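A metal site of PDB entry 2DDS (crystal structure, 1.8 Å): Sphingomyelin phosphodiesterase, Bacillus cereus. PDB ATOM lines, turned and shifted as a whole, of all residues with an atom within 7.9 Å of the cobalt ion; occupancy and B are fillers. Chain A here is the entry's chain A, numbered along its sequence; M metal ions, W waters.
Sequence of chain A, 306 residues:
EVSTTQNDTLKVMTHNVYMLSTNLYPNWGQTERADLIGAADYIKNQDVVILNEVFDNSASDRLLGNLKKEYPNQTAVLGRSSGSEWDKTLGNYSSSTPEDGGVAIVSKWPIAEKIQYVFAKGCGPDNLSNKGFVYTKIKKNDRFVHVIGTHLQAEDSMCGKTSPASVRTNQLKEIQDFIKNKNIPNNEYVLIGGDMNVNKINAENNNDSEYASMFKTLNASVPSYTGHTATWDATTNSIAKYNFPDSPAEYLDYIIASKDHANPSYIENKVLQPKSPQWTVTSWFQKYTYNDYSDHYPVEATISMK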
ATOM      1  N   MET A  19      -5.391 -21.374   7.046  1.00  0.00           N
ATOM      2  CA  MET A  19      -5.795 -22.562   6.310  1.00  0.00           C
ATOM      3  C   MET A  19      -7.224 -22.937   6.665  1.00  0.00           C
ATOM      4  O   MET A  19      -7.476 -23.897   7.392  1.00  0.00           O
ATOM      5  CB  MET A  19      -4.869 -23.735   6.608  1.00  0.00           C
ATOM      6  CG  MET A  19      -3.481 -23.528   6.075  1.00  0.00           C
ATOM      7  SD  MET A  19      -2.563 -25.061   6.008  1.00  0.00           S
ATOM      8  CE  MET A  19      -1.416 -24.703   4.674  1.00  0.00           C
ATOM      9  N   LEU A  20      -8.162 -22.140   6.152  1.00  0.00           N
ATOM     10  CA  LEU A  20      -9.573 -22.380   6.405  1.00  0.00           C
ATOM     11  C   LEU A  20      -9.974 -23.679   5.732  1.00  0.00           C
ATOM     12  O   LEU A  20      -9.321 -24.136   4.793  1.00  0.00           O
ATOM     13  CB  LEU A  20     -10.404 -21.224   5.842  1.00  0.00           C
ATOM     14  CG  LEU A  20     -10.057 -19.847   6.418  1.00  0.00           C
ATOM     15  CD1 LEU A  20     -10.914 -18.784   5.753  1.00  0.00           C
ATOM     16  CD2 LEU A  20     -10.263 -19.864   7.928  1.00  0.00           C
ATOM     17  N   SER A  21     -11.051 -24.286   6.216  1.00  0.00           N
ATOM     18  CA  SER A  21     -11.543 -25.531   5.624  1.00  0.00           C
ATOM     19  C   SER A  21     -11.909 -25.325   4.162  1.00  0.00           C
ATOM     20  O   SER A  21     -12.619 -24.374   3.822  1.00  0.00           O
ATOM     21  CB  SER A  21     -12.766 -26.034   6.377  1.00  0.00           C
ATOM     22  OG  SER A  21     -13.389 -27.085   5.670  1.00  0.00           O
ATOM     23  N   VAL A  54      -4.659 -23.979  11.309  1.00  0.00           N
ATOM     24  CA  VAL A  54      -4.426 -25.153  10.471  1.00  0.00           C
ATOM     25  C   VAL A  54      -5.728 -25.949  10.581  1.00  0.00           C
ATOM     26  O   VAL A  54      -5.761 -27.084  11.057  1.00  0.00           O
ATOM     27  CB  VAL A  54      -3.214 -26.006  10.939  1.00  0.00           C
ATOM     28  CG1 VAL A  54      -1.930 -25.286  10.556  1.00  0.00           C
ATOM     29  CG2 VAL A  54      -3.264 -26.245  12.440  1.00  0.00           C
ATOM     30  N   PHE A  55      -6.816 -25.312  10.129  1.00  0.00           N
ATOM     31  CA  PHE A  55      -8.172 -25.865  10.151  1.00  0.00           C
ATOM     32  C   PHE A  55      -8.429 -26.967   9.130  1.00  0.00           C
ATOM     33  O   PHE A  55      -8.897 -28.052   9.478  1.00  0.00           O
ATOM     34  CB  PHE A  55      -9.206 -24.754   9.929  1.00  0.00           C
ATOM     35  CG  PHE A  55      -9.259 -23.733  11.041  1.00  0.00           C
ATOM     36  CD1 PHE A  55      -9.112 -22.383  10.759  1.00  0.00           C
ATOM     37  CD2 PHE A  55      -9.502 -24.118  12.350  1.00  0.00           C
ATOM     38  CE1 PHE A  55      -9.195 -21.423  11.774  1.00  0.00           C
ATOM     39  CE2 PHE A  55      -9.581 -23.178  13.378  1.00  0.00           C
ATOM     40  CZ  PHE A  55      -9.427 -21.825  13.084  1.00  0.00           C
ATOM     41  N   ASP A  56      -8.142 -26.693   7.864  1.00  0.00           N
ATOM     42  CA  ASP A  56      -8.396 -27.700   6.844  1.00  0.00           C
ATOM     43  C   ASP A  56      -7.635 -28.972   7.195  1.00  0.00           C
ATOM     44  O   ASP A  56      -6.408 -28.953   7.313  1.00  0.00           O
ATOM     45  CB  ASP A  56      -7.951 -27.204   5.472  1.00  0.00           C
ATOM     46  CG  ASP A  56      -8.394 -28.121   4.369  1.00  0.00           C
ATOM     47  OD1 ASP A  56      -9.611 -28.191   4.113  1.00  0.00           O
ATOM     48  OD2 ASP A  56      -7.524 -28.797   3.771  1.00  0.00           O
ATOM     49  N   ASN A  57      -8.351 -30.072   7.347  1.00  0.00           N
ATOM     50  CA  ASN A  57      -7.707 -31.334   7.731  1.00  0.00           C
ATOM     51  C   ASN A  57      -6.667 -31.824   6.729  1.00  0.00           C
ATOM     52  O   ASN A  57      -5.548 -32.160   7.126  1.00  0.00           O
ATOM     53  CB  ASN A  57      -8.762 -32.415   7.959  1.00  0.00           C
ATOM     54  CG  ASN A  57      -9.667 -32.102   9.123  1.00  0.00           C
ATOM     55  OD1 ASN A  57      -9.543 -31.039   9.733  1.00  0.00           O
ATOM     56  ND2 ASN A  57     -10.580 -33.007   9.445  1.00  0.00           N
ATOM     57  N   SER A  58      -7.018 -31.867   5.448  1.00  0.00           N
ATOM     58  CA  SER A  58      -6.086 -32.344   4.435  1.00  0.00           C
ATOM     59  C   SER A  58      -4.845 -31.471   4.282  1.00  0.00           C
ATOM     60  O   SER A  58      -3.723 -31.986   4.276  1.00  0.00           O
ATOM     61  CB  SER A  58      -6.793 -32.462   3.076  1.00  0.00           C
ATOM     62  OG  SER A  58      -7.740 -33.515   3.090  1.00  0.00           O
ATOM     63  N   SER A  60      -3.670 -29.213   6.407  1.00  0.00           N
ATOM     64  CA  SER A  60      -2.890 -29.104   7.640  1.00  0.00           C
ATOM     65  C   SER A  60      -1.991 -30.327   7.797  1.00  0.00           C
ATOM     66  O   SER A  60      -0.829 -30.201   8.178  1.00  0.00           O
ATOM     67  CB  SER A  60      -3.805 -28.947   8.857  1.00  0.00           C
ATOM     68  OG  SER A  60      -4.617 -30.091   9.079  1.00  0.00           O
ATOM     69  N   VAL A  77      -3.599 -31.742  15.945  1.00  0.00           N
ATOM     70  CA  VAL A  77      -4.200 -30.432  15.897  1.00  0.00           C
ATOM     71  C   VAL A  77      -5.273 -30.312  16.967  1.00  0.00           C
ATOM     72  O   VAL A  77      -6.168 -31.160  17.076  1.00  0.00           O
ATOM     73  CB  VAL A  77      -4.834 -30.140  14.516  1.00  0.00           C
ATOM     74  CG1 VAL A  77      -5.539 -28.773  14.519  1.00  0.00           C
ATOM     75  CG2 VAL A  77      -3.745 -30.143  13.451  1.00  0.00           C
ATOM     76  N   LEU A  78      -5.168 -29.261  17.760  1.00  0.00           N
ATOM     77  CA  LEU A  78      -6.112 -28.978  18.823  1.00  0.00           C
ATOM     78  C   LEU A  78      -7.556 -29.235  18.411  1.00  0.00           C
ATOM     79  O   LEU A  78      -7.994 -28.776  17.351  1.00  0.00           O
ATOM     80  CB  LEU A  78      -5.980 -27.509  19.238  1.00  0.00           C
ATOM     81  CG  LEU A  78      -7.055 -26.939  20.169  1.00  0.00           C
ATOM     82  CD1 LEU A  78      -6.923 -27.605  21.549  1.00  0.00           C
ATOM     83  CD2 LEU A  78      -6.917 -25.428  20.273  1.00  0.00           C
ATOM     84  N   GLY A  79      -8.290 -29.958  19.252  1.00  0.00           N
ATOM     85  CA  GLY A  79      -9.695 -30.216  18.998  1.00  0.00           C
ATOM     86  C   GLY A  79     -10.151 -31.097  17.850  1.00  0.00           C
ATOM     87  O   GLY A  79     -11.343 -31.130  17.550  1.00  0.00           O
ATOM     88  N   ARG A  80      -9.227 -31.801  17.215  1.00  0.00           N
ATOM     89  CA  ARG A  80      -9.606 -32.657  16.087  1.00  0.00           C
ATOM     90  C   ARG A  80      -9.886 -34.089  16.558  1.00  0.00           C
ATOM     91  O   ARG A  80     -10.670 -34.809  15.934  1.00  0.00           O
ATOM     92  CB  ARG A  80      -8.502 -32.661  15.031  1.00  0.00           C
ATOM     93  CG  ARG A  80      -8.895 -33.348  13.727  1.00  0.00           C
ATOM     94  CD  ARG A  80      -7.848 -33.129  12.649  1.00  0.00           C
ATOM     95  NE  ARG A  80      -7.709 -31.718  12.305  1.00  0.00           N
ATOM     96  CZ  ARG A  80      -6.729 -31.238  11.543  1.00  0.00           C
ATOM     97  NH1 ARG A  80      -5.806 -32.063  11.057  1.00  0.00           N
ATOM     98  NH2 ARG A  80      -6.675 -29.935  11.258  1.00  0.00           N
ATOM     99  N   PRO A  98     -18.172 -28.521  14.422  1.00  0.00           N
ATOM    100  CA  PRO A  98     -18.010 -28.528  12.956  1.00  0.00           C
ATOM    101  C   PRO A  98     -16.550 -28.399  12.538  1.00  0.00           C
ATOM    102  O   PRO A  98     -16.177 -28.851  11.458  1.00  0.00           O
ATOM    103  CB  PRO A  98     -18.846 -27.320  12.519  1.00  0.00           C
ATOM    104  CG  PRO A  98     -19.881 -27.200  13.591  1.00  0.00           C
ATOM    105  CD  PRO A  98     -19.084 -27.435  14.835  1.00  0.00           C
ATOM    106  N   GLU A  99     -15.738 -27.787  13.386  1.00  0.00           N
ATOM    107  CA  GLU A  99     -14.326 -27.562  13.073  1.00  0.00           C
ATOM    108  C   GLU A  99     -13.414 -27.738  14.292  1.00  0.00           C
ATOM    109  O   GLU A  99     -13.870 -27.701  15.428  1.00  0.00           O
ATOM    110  CB  GLU A  99     -14.180 -26.150  12.488  1.00  0.00           C
ATOM    111  CG  GLU A  99     -12.794 -25.763  12.025  1.00  0.00           C
ATOM    112  CD  GLU A  99     -12.246 -26.716  10.996  1.00  0.00           C
ATOM    113  OE1 GLU A  99     -11.372 -27.528  11.359  1.00  0.00           O
ATOM    114  OE2 GLU A  99     -12.701 -26.664   9.833  1.00  0.00           O
ATOM    115  N   ASP A 100     -12.124 -27.939  14.045  1.00  0.00           N
ATOM    116  CA  ASP A 100     -11.167 -28.096  15.137  1.00  0.00           C
ATOM    117  C   ASP A 100     -10.608 -26.728  15.526  1.00  0.00           C
ATOM    118  O   ASP A 100     -10.957 -25.722  14.903  1.00  0.00           O
ATOM    119  CB  ASP A 100     -10.034 -29.055  14.748  1.00  0.00           C
ATOM    120  CG  ASP A 100      -9.330 -28.639  13.463  1.00  0.00           C
ATOM    121  OD1 ASP A 100      -8.721 -27.550  13.449  1.00  0.00           O
ATOM    122  OD2 ASP A 100      -9.377 -29.407  12.479  1.00  0.00           O
ATOM    123  N   GLY A 101      -9.759 -26.708  16.543  1.00  0.00           N
ATOM    124  CA  GLY A 101      -9.165 -25.465  17.031  1.00  0.00           C
ATOM    125  C   GLY A 101      -8.060 -24.866  16.169  1.00  0.00           C
ATOM    126  O   GLY A 101      -7.650 -23.720  16.392  1.00  0.00           O
ATOM    127  N   GLY A 102      -7.573 -25.640  15.212  1.00  0.00           N
ATOM    128  CA  GLY A 102      -6.546 -25.151  14.314  1.00  0.00           C
ATOM    129  C   GLY A 102      -5.193 -24.809  14.905  1.00  0.00           C
ATOM    130  O   GLY A 102      -4.405 -24.073  14.289  1.00  0.00           O
ATOM    131  N   SER A 129     -15.853 -24.915  17.361  1.00  0.00           N
ATOM    132  CA  SER A 129     -14.506 -25.054  16.800  1.00  0.00           C
ATOM    133  C   SER A 129     -13.425 -25.494  17.786  1.00  0.00           C
ATOM    134  O   SER A 129     -12.253 -25.516  17.436  1.00  0.00           O
ATOM    135  CB  SER A 129     -14.099 -23.731  16.148  1.00  0.00           C
ATOM    136  OG  SER A 129     -12.951 -23.894  15.341  1.00  0.00           O
HETATM  137 CO    CO M   1     -10.438 -29.179  10.595  1.00  0.00          CO
HETATM  138  O   HOH W   1     -11.999 -30.521  11.508  1.00  0.00           O
HETATM  139  O   HOH W   2     -11.612 -28.915   8.727  1.00  0.00           O
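The cobalt ion is bound by the side-chain carboxylate of Glu 99 (2.0 Å), the side-chain carboxylate of Asp 100 (2.2 Å), the backbone carbonyl oxygen of Phe 55 (2.2 Å), water W2 (2.2 Å), the side-chain amide oxygen of Asn 57 (2.2 Å) and water W1 (2.3 Å).
OD1 of Asn 57 lies close to NE of Arg 80, 3.2 Å away.
NH2 of Arg 80 lies close to O of Phe 55, at 3.4 Å.
O of Asn 57 sits at hydrogen-bond distance from OG of Ser 60 (3.0 Å).
The side-chain carboxylate of Asp 100 is in hydrogen-bond range of the backbone NH of Gly 102 (2.8 Å).
The side-chain carboxylate (OD1) of Asp 100 is in salt-bridge range of the guanidinium group (NH2) of Arg 80, 3.8 Å away.
The backbone NH (N) of Phe 55 sits at hydrogen-bond distance from the backbone carbonyl oxygen (O) of Met 19 (3.2 Å).
The guanidinium group of Arg 80 sits at hydrogen-bond distance from the side-chain hydroxyl of Ser 60 (3.0 Å).
O of Val 54 is in hydrogen-bond range of NH2 of Arg 80, at 3.0 Å.
Residues that only touch the cobalt ion: Arg 80 (3.9 Å).
Within 4 Å of the cobalt ion: Phe 55, Asn 57, Arg 80, Glu 99 and Asp 100.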
